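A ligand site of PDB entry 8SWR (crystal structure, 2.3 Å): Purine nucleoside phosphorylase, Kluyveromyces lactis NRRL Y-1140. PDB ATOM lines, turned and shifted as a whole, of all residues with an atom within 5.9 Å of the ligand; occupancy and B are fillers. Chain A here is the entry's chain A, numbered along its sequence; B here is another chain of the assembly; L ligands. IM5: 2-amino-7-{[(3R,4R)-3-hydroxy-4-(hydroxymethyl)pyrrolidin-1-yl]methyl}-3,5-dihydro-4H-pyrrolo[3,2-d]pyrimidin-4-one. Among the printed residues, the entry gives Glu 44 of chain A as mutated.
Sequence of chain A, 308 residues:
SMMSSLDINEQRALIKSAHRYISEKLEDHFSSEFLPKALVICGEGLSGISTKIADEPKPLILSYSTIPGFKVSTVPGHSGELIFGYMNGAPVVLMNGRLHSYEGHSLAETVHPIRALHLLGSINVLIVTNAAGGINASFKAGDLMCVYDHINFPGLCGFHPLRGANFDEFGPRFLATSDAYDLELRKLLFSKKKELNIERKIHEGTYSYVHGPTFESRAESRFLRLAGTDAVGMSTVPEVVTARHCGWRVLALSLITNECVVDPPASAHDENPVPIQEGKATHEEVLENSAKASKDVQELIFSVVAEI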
ATOM      1  N   GLU A  44      17.153 -10.209 -18.066  1.00  0.00           N
ATOM      2  CA  GLU A  44      17.141  -9.244 -19.158  1.00  0.00           C
ATOM      3  C   GLU A  44      15.966  -9.557 -20.078  1.00  0.00           C
ATOM      4  O   GLU A  44      15.834 -10.685 -20.573  1.00  0.00           O
ATOM      5  CB  GLU A  44      18.455  -9.282 -19.925  1.00  0.00           C
ATOM      6  CG  GLU A  44      18.609  -8.139 -20.925  1.00  0.00           C
ATOM      7  CD  GLU A  44      19.861  -8.264 -21.764  1.00  0.00           C
ATOM      8  OE1 GLU A  44      20.359  -9.402 -21.930  1.00  0.00           O
ATOM      9  OE2 GLU A  44      20.349  -7.232 -22.259  1.00  0.00           O
ATOM     10  N   HIS A 100      26.652  -9.409 -13.732  1.00  0.00           N
ATOM     11  CA  HIS A 100      27.185 -10.629 -14.314  1.00  0.00           C
ATOM     12  C   HIS A 100      28.700 -10.655 -14.179  1.00  0.00           C
ATOM     13  O   HIS A 100      29.366  -9.614 -14.171  1.00  0.00           O
ATOM     14  CB  HIS A 100      26.808 -10.754 -15.799  1.00  0.00           C
ATOM     15  CG  HIS A 100      25.377 -10.426 -16.094  1.00  0.00           C
ATOM     16  ND1 HIS A 100      24.422 -11.390 -16.325  1.00  0.00           N
ATOM     17  CD2 HIS A 100      24.741  -9.228 -16.206  1.00  0.00           C
ATOM     18  CE1 HIS A 100      23.263 -10.801 -16.563  1.00  0.00           C
ATOM     19  NE2 HIS A 100      23.425  -9.495 -16.496  1.00  0.00           N
ATOM     20  N   TYR A 102      30.876 -11.832 -16.297  1.00  0.00           N
ATOM     21  CA  TYR A 102      31.582 -11.475 -17.529  1.00  0.00           C
ATOM     22  C   TYR A 102      31.763  -9.976 -17.694  1.00  0.00           C
ATOM     23  O   TYR A 102      32.546  -9.555 -18.551  1.00  0.00           O
ATOM     24  CB  TYR A 102      30.852 -12.060 -18.742  1.00  0.00           C
ATOM     25  CG  TYR A 102      29.397 -11.672 -18.900  1.00  0.00           C
ATOM     26  CD1 TYR A 102      29.028 -10.342 -19.130  1.00  0.00           C
ATOM     27  CD2 TYR A 102      28.383 -12.614 -18.818  1.00  0.00           C
ATOM     28  CE1 TYR A 102      27.695  -9.986 -19.279  1.00  0.00           C
ATOM     29  CE2 TYR A 102      27.056 -12.267 -18.959  1.00  0.00           C
ATOM     30  CZ  TYR A 102      26.719 -10.953 -19.194  1.00  0.00           C
ATOM     31  OH  TYR A 102      25.397 -10.584 -19.336  1.00  0.00           O
ATOM     32  N   ASN A 130      15.659 -15.901 -15.578  1.00  0.00           N
ATOM     33  CA  ASN A 130      16.758 -15.683 -16.516  1.00  0.00           C
ATOM     34  C   ASN A 130      16.334 -16.168 -17.901  1.00  0.00           C
ATOM     35  O   ASN A 130      15.289 -16.800 -18.069  1.00  0.00           O
ATOM     36  CB  ASN A 130      18.039 -16.414 -16.074  1.00  0.00           C
ATOM     37  CG  ASN A 130      17.818 -17.901 -15.806  1.00  0.00           C
ATOM     38  OD1 ASN A 130      17.801 -18.336 -14.663  1.00  0.00           O
ATOM     39  ND2 ASN A 130      17.676 -18.677 -16.879  1.00  0.00           N
ATOM     40  N   ALA A 131      17.161 -15.842 -18.879  1.00  0.00           N
ATOM     41  CA  ALA A 131      17.097 -16.447 -20.202  1.00  0.00           C
ATOM     42  C   ALA A 131      18.100 -17.583 -20.268  1.00  0.00           C
ATOM     43  O   ALA A 131      19.081 -17.628 -19.528  1.00  0.00           O
ATOM     44  CB  ALA A 131      17.378 -15.413 -21.290  1.00  0.00           C
ATOM     45  N   ALA A 132      17.842 -18.527 -21.180  1.00  0.00           N
ATOM     46  CA  ALA A 132      18.702 -19.696 -21.254  1.00  0.00           C
ATOM     47  C   ALA A 132      18.584 -20.343 -22.627  1.00  0.00           C
ATOM     48  O   ALA A 132      17.511 -20.335 -23.235  1.00  0.00           O
ATOM     49  CB  ALA A 132      18.333 -20.718 -20.163  1.00  0.00           C
ATOM     50  N   GLY A 133      19.706 -20.885 -23.108  1.00  0.00           N
ATOM     51  CA  GLY A 133      19.672 -21.722 -24.283  1.00  0.00           C
ATOM     52  C   GLY A 133      19.219 -23.131 -23.949  1.00  0.00           C
ATOM     53  O   GLY A 133      19.462 -23.648 -22.860  1.00  0.00           O
ATOM     54  N   GLY A 134      18.554 -23.765 -24.914  1.00  0.00           N
ATOM     55  CA  GLY A 134      18.028 -25.096 -24.690  1.00  0.00           C
ATOM     56  C   GLY A 134      18.997 -26.202 -25.058  1.00  0.00           C
ATOM     57  O   GLY A 134      19.328 -26.378 -26.236  1.00  0.00           O
ATOM     58  N   VAL A 210      27.258 -21.134 -16.806  1.00  0.00           N
ATOM     59  CA  VAL A 210      28.561 -20.913 -17.413  1.00  0.00           C
ATOM     60  C   VAL A 210      28.842 -19.417 -17.399  1.00  0.00           C
ATOM     61  O   VAL A 210      27.928 -18.587 -17.279  1.00  0.00           O
ATOM     62  CB  VAL A 210      28.648 -21.469 -18.847  1.00  0.00           C
ATOM     63  CG1 VAL A 210      28.345 -22.970 -18.864  1.00  0.00           C
ATOM     64  CG2 VAL A 210      27.695 -20.726 -19.765  1.00  0.00           C
ATOM     65  N   THR A 214      30.607 -15.585 -24.316  1.00  0.00           N
ATOM     66  CA  THR A 214      30.413 -16.312 -25.561  1.00  0.00           C
ATOM     67  C   THR A 214      29.238 -17.269 -25.468  1.00  0.00           C
ATOM     68  O   THR A 214      28.999 -17.865 -24.408  1.00  0.00           O
ATOM     69  CB  THR A 214      31.672 -17.094 -25.943  1.00  0.00           C
ATOM     70  OG1 THR A 214      32.166 -17.816 -24.805  1.00  0.00           O
ATOM     71  CG2 THR A 214      32.752 -16.179 -26.492  1.00  0.00           C
ATOM     72  N   PHE A 215      28.503 -17.402 -26.560  1.00  0.00           N
ATOM     73  CA  PHE A 215      27.572 -18.517 -26.672  1.00  0.00           C
ATOM     74  C   PHE A 215      28.365 -19.802 -26.875  1.00  0.00           C
ATOM     75  O   PHE A 215      29.510 -19.792 -27.342  1.00  0.00           O
ATOM     76  CB  PHE A 215      26.592 -18.298 -27.822  1.00  0.00           C
ATOM     77  CG  PHE A 215      25.573 -17.214 -27.554  1.00  0.00           C
ATOM     78  CD1 PHE A 215      24.536 -17.432 -26.660  1.00  0.00           C
ATOM     79  CD2 PHE A 215      25.650 -15.993 -28.197  1.00  0.00           C
ATOM     80  CE1 PHE A 215      23.599 -16.442 -26.417  1.00  0.00           C
ATOM     81  CE2 PHE A 215      24.713 -15.003 -27.954  1.00  0.00           C
ATOM     82  CZ  PHE A 215      23.687 -15.227 -27.064  1.00  0.00           C
ATOM     83  N   GLU A 216      27.756 -20.922 -26.519  1.00  0.00           N
ATOM     84  CA  GLU A 216      28.479 -22.184 -26.487  1.00  0.00           C
ATOM     85  C   GLU A 216      28.823 -22.645 -27.894  1.00  0.00           C
ATOM     86  O   GLU A 216      28.039 -22.495 -28.829  1.00  0.00           O
ATOM     87  CB  GLU A 216      27.648 -23.258 -25.783  1.00  0.00           C
ATOM     88  CG  GLU A 216      27.556 -23.086 -24.284  1.00  0.00           C
ATOM     89  CD  GLU A 216      26.702 -21.892 -23.892  1.00  0.00           C
ATOM     90  OE1 GLU A 216      25.862 -21.462 -24.707  1.00  0.00           O
ATOM     91  OE2 GLU A 216      26.883 -21.390 -22.763  1.00  0.00           O
ATOM     92  N   VAL A 232      21.195 -23.861 -20.419  1.00  0.00           N
ATOM     93  CA  VAL A 232      22.460 -23.213 -20.060  1.00  0.00           C
ATOM     94  C   VAL A 232      22.260 -21.710 -20.070  1.00  0.00           C
ATOM     95  O   VAL A 232      21.675 -21.156 -21.002  1.00  0.00           O
ATOM     96  CB  VAL A 232      23.599 -23.631 -21.013  1.00  0.00           C
ATOM     97  CG1 VAL A 232      23.218 -23.376 -22.464  1.00  0.00           C
ATOM     98  CG2 VAL A 232      24.877 -22.904 -20.654  1.00  0.00           C
ATOM     99  N   GLY A 233      22.740 -21.053 -19.016  1.00  0.00           N
ATOM    100  CA  GLY A 233      22.674 -19.607 -18.923  1.00  0.00           C
ATOM    101  C   GLY A 233      23.926 -19.025 -18.317  1.00  0.00           C
ATOM    102  O   GLY A 233      24.917 -19.738 -18.097  1.00  0.00           O
ATOM    103  N   MET A 234      23.907 -17.717 -18.022  1.00  0.00           N
ATOM    104  CA  MET A 234      25.093 -16.999 -17.548  1.00  0.00           C
ATOM    105  C   MET A 234      24.871 -16.367 -16.181  1.00  0.00           C
ATOM    106  O   MET A 234      25.625 -15.459 -15.800  1.00  0.00           O
ATOM    107  CB  MET A 234      25.485 -15.938 -18.572  1.00  0.00           C
ATOM    108  CG  MET A 234      26.008 -16.524 -19.880  1.00  0.00           C
ATOM    109  SD  MET A 234      26.638 -15.261 -21.002  1.00  0.00           S
ATOM    110  CE  MET A 234      26.553 -16.121 -22.570  1.00  0.00           C
ATOM    111  N   LEU A 255      13.858 -19.055 -18.987  1.00  0.00           N
ATOM    112  CA  LEU A 255      13.186 -18.761 -20.242  1.00  0.00           C
ATOM    113  C   LEU A 255      14.033 -19.300 -21.386  1.00  0.00           C
ATOM    114  O   LEU A 255      15.165 -18.855 -21.588  1.00  0.00           O
ATOM    115  CB  LEU A 255      12.936 -17.254 -20.393  1.00  0.00           C
ATOM    116  CG  LEU A 255      11.490 -16.808 -20.524  1.00  0.00           C
ATOM    117  CD1 LEU A 255      11.414 -15.325 -20.816  1.00  0.00           C
ATOM    118  CD2 LEU A 255      10.921 -17.581 -21.701  1.00  0.00           C
ATOM    119  N   THR A 257      15.206 -19.217 -24.702  1.00  0.00           N
ATOM    120  CA  THR A 257      15.240 -18.213 -25.757  1.00  0.00           C
ATOM    121  C   THR A 257      15.849 -18.719 -27.056  1.00  0.00           C
ATOM    122  O   THR A 257      15.715 -18.057 -28.085  1.00  0.00           O
ATOM    123  CB  THR A 257      16.023 -16.979 -25.286  1.00  0.00           C
ATOM    124  OG1 THR A 257      17.341 -17.368 -24.874  1.00  0.00           O
ATOM    125  CG2 THR A 257      15.307 -16.309 -24.140  1.00  0.00           C
ATOM    126  N   ASN A 258      16.507 -19.879 -27.036  1.00  0.00           N
ATOM    127  CA  ASN A 258      17.118 -20.423 -28.247  1.00  0.00           C
ATOM    128  C   ASN A 258      17.447 -21.886 -28.003  1.00  0.00           C
ATOM    129  O   ASN A 258      17.511 -22.349 -26.855  1.00  0.00           O
ATOM    130  CB  ASN A 258      18.376 -19.654 -28.649  1.00  0.00           C
ATOM    131  CG  ASN A 258      19.399 -19.587 -27.539  1.00  0.00           C
ATOM    132  OD1 ASN A 258      19.157 -18.941 -26.518  1.00  0.00           O
ATOM    133  ND2 ASN A 258      20.533 -20.238 -27.723  1.00  0.00           N
ATOM    134  N   CYS A 260      20.298 -24.470 -28.455  1.00  0.00           N
ATOM    135  CA  CYS A 260      21.741 -24.566 -28.679  1.00  0.00           C
ATOM    136  C   CYS A 260      22.055 -25.521 -29.819  1.00  0.00           C
ATOM    137  O   CYS A 260      21.431 -26.580 -29.964  1.00  0.00           O
ATOM    138  CB  CYS A 260      22.437 -25.050 -27.402  1.00  0.00           C
ATOM    139  SG  CYS A 260      22.180 -23.990 -25.956  1.00  0.00           S
ATOM    140  N   ALA A 281      23.321 -18.559 -32.369  1.00  0.00           N
ATOM    141  CA  ALA A 281      22.677 -17.739 -31.361  1.00  0.00           C
ATOM    142  C   ALA A 281      23.032 -16.270 -31.566  1.00  0.00           C
ATOM    143  O   ALA A 281      24.148 -15.934 -31.960  1.00  0.00           O
ATOM    144  CB  ALA A 281      23.099 -18.195 -29.963  1.00  0.00           C
ATOM    145  N   THR A 282      22.053 -15.395 -31.322  1.00  0.00           N
ATOM    146  CA  THR A 282      22.266 -13.957 -31.351  1.00  0.00           C
ATOM    147  C   THR A 282      21.679 -13.347 -30.090  1.00  0.00           C
ATOM    148  O   THR A 282      20.794 -13.931 -29.453  1.00  0.00           O
ATOM    149  CB  THR A 282      21.649 -13.303 -32.592  1.00  0.00           C
ATOM    150  OG1 THR A 282      20.222 -13.306 -32.473  1.00  0.00           O
ATOM    151  CG2 THR A 282      22.048 -14.029 -33.870  1.00  0.00           C
ATOM    152  N   HIS A 283      22.174 -12.160 -29.736  1.00  0.00           N
ATOM    153  CA  HIS A 283      21.608 -11.454 -28.592  1.00  0.00           C
ATOM    154  C   HIS A 283      20.229 -10.900 -28.922  1.00  0.00           C
ATOM    155  O   HIS A 283      19.345 -10.870 -28.058  1.00  0.00           O
ATOM    156  CB  HIS A 283      22.556 -10.334 -28.145  1.00  0.00           C
ATOM    157  CG  HIS A 283      22.133  -9.654 -26.881  1.00  0.00           C
ATOM    158  ND1 HIS A 283      21.729 -10.340 -25.750  1.00  0.00           N
ATOM    159  CD2 HIS A 283      22.006  -8.339 -26.585  1.00  0.00           C
ATOM    160  CE1 HIS A 283      21.404  -9.478 -24.810  1.00  0.00           C
ATOM    161  NE2 HIS A 283      21.560  -8.251 -25.297  1.00  0.00           N
ATOM    162  N   VAL A 286      17.673 -13.488 -28.243  1.00  0.00           N
ATOM    163  CA  VAL A 286      17.389 -13.712 -26.838  1.00  0.00           C
ATOM    164  C   VAL A 286      16.488 -12.608 -26.290  1.00  0.00           C
ATOM    165  O   VAL A 286      15.517 -12.877 -25.577  1.00  0.00           O
ATOM    166  CB  VAL A 286      18.689 -13.818 -26.024  1.00  0.00           C
ATOM    167  CG1 VAL A 286      18.344 -14.029 -24.572  1.00  0.00           C
ATOM    168  CG2 VAL A 286      19.554 -14.942 -26.546  1.00  0.00           C
ATOM    169  N   LEU A 287      16.804 -11.346 -26.617  1.00  0.00           N
ATOM    170  CA  LEU A 287      15.982 -10.245 -26.153  1.00  0.00           C
ATOM    171  C   LEU A 287      14.555 -10.364 -26.672  1.00  0.00           C
ATOM    172  O   LEU A 287      13.590 -10.155 -25.938  1.00  0.00           O
ATOM    173  CB  LEU A 287      16.587  -8.905 -26.594  1.00  0.00           C
ATOM    174  CG  LEU A 287      17.950  -8.492 -26.065  1.00  0.00           C
ATOM    175  CD1 LEU A 287      18.470  -7.332 -26.880  1.00  0.00           C
ATOM    176  CD2 LEU A 287      17.852  -8.120 -24.600  1.00  0.00           C
ATOM    177  N   PHE B 174      27.954 -10.369 -26.862  1.00  0.00           N
ATOM    178  CA  PHE B 174      27.740 -11.808 -26.832  1.00  0.00           C
ATOM    179  C   PHE B 174      28.080 -12.376 -28.195  1.00  0.00           C
ATOM    180  O   PHE B 174      27.414 -12.063 -29.190  1.00  0.00           O
ATOM    181  CB  PHE B 174      26.311 -12.144 -26.420  1.00  0.00           C
ATOM    182  CG  PHE B 174      25.888 -11.465 -25.156  1.00  0.00           C
ATOM    183  CD1 PHE B 174      26.339 -11.920 -23.935  1.00  0.00           C
ATOM    184  CD2 PHE B 174      25.033 -10.373 -25.177  1.00  0.00           C
ATOM    185  CE1 PHE B 174      25.964 -11.294 -22.756  1.00  0.00           C
ATOM    186  CE2 PHE B 174      24.651  -9.751 -24.011  1.00  0.00           C
ATOM    187  CZ  PHE B 174      25.113 -10.212 -22.794  1.00  0.00           C
HETATM  188  N1  IM5 L   1      23.761 -19.800 -23.772  1.00  0.00           N
HETATM  189  C2  IM5 L   1      24.096 -19.174 -22.592  1.00  0.00           C
HETATM  190  N2  IM5 L   1      25.255 -19.537 -22.022  1.00  0.00           N
HETATM  191  N3  IM5 L   1      23.331 -18.272 -22.031  1.00  0.00           N
HETATM  192  C4  IM5 L   1      22.169 -17.958 -22.669  1.00  0.00           C
HETATM  193  C5  IM5 L   1      21.780 -18.561 -23.868  1.00  0.00           C
HETATM  194  C6  IM5 L   1      22.596 -19.547 -24.482  1.00  0.00           C
HETATM  195  O6  IM5 L   1      22.376 -20.149 -25.533  1.00  0.00           O
HETATM  196  N7  IM5 L   1      20.570 -18.007 -24.209  1.00  0.00           N
HETATM  197  C8  IM5 L   1      20.223 -17.104 -23.253  1.00  0.00           C
HETATM  198  C9  IM5 L   1      21.202 -17.049 -22.308  1.00  0.00           C
HETATM  199  N1' IM5 L   1      21.872 -14.905 -21.235  1.00  0.00           N
HETATM  200  C10 IM5 L   1      21.233 -16.214 -21.072  1.00  0.00           C
HETATM  201  C2' IM5 L   1      23.049 -14.927 -22.115  1.00  0.00           C
HETATM  202  C3' IM5 L   1      23.315 -13.454 -22.288  1.00  0.00           C
HETATM  203  O3' IM5 L   1      23.879 -12.907 -21.111  1.00  0.00           O
HETATM  204  C4' IM5 L   1      21.905 -12.911 -22.570  1.00  0.00           C
HETATM  205  C5' IM5 L   1      21.581 -12.836 -24.047  1.00  0.00           C
HETATM  206  O5' IM5 L   1      22.749 -12.848 -24.849  1.00  0.00           O
HETATM  207  C6' IM5 L   1      20.983 -13.889 -21.821  1.00  0.00           C
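NE2 of His 283 sits at hydrogen-bond distance from OE2 of Glu 44 (3.4 Å). The side-chain hydroxyl (OG1) of Thr 257 lies within hydrogen-bond range of the side-chain amide oxygen (OD1) of Asn 258 (2.9 Å). The backbone carbonyl oxygen of Asn 258 is in hydrogen-bond range of the backbone NH of Gly 134 (2.6 Å). The backbone carbonyl oxygen of Val 232 is in hydrogen-bond range of the backbone NH of Gly 133 (2.9 Å). A ring nitrogen (ND1) of His 100 sits close to the side-chain hydroxyl of Tyr 102 (3.3 Å). The backbone carbonyl oxygen of Gly 233 sits at hydrogen-bond distance from the backbone NH of Val 210. The backbone NH (N) of Ala 132 lies within hydrogen-bond range of the backbone carbonyl oxygen (O) of Leu 255 (2.7 Å). O of Gly 134 lies within hydrogen-bond range of N of Cys 260 (3.1 Å).
OE1 of Glu 44 touches C4' of the ligand, 3.9 Å away. O of Ala 131 touches C10 of the ligand (3.0 Å). Ala 132 touches the ligand (C to N7, 3.5 Å). CG2 of Val 210 touches N2 of the ligand, 3.5 Å away. Phe 215 touches the ligand (CZ to O5', 3.4 Å). Gly 233 touches the ligand. SG of Cys 260 touches O6 of the ligand (3.9 Å). Val 286 touches the ligand. Phe 174 of chain B touches the ligand. The nearest printed residue that does not touch the ligand is Thr 214 (4.7 Å).
N2 of the ligand sits at hydrogen-bond distance from OE2 of Glu 216, 2.6 Å away. A ring nitrogen (ND1) of His 283 lies within hydrogen-bond range of an oxygen (O5') of the ligand, 2.9 Å away. ND2 of Asn 258 sits at hydrogen-bond distance from O6 of the ligand (2.9 Å). The backbone NH (N) of Gly 133 lies close to a nitrogen (N7) of the ligand, 3.2 Å away. O3' of the ligand lies within hydrogen-bond range of OH of Tyr 102 (3.3 Å). A nitrogen (N7) of the ligand lies close to the side-chain hydroxyl (OG1) of Thr 257 (3.4 Å). The backbone carbonyl oxygen of Val 232 lies close to a nitrogen (N3) of the ligand (3.5 Å). SD of Met 234 lies within hydrogen-bond range of O3' of the ligand (3.6 Å).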
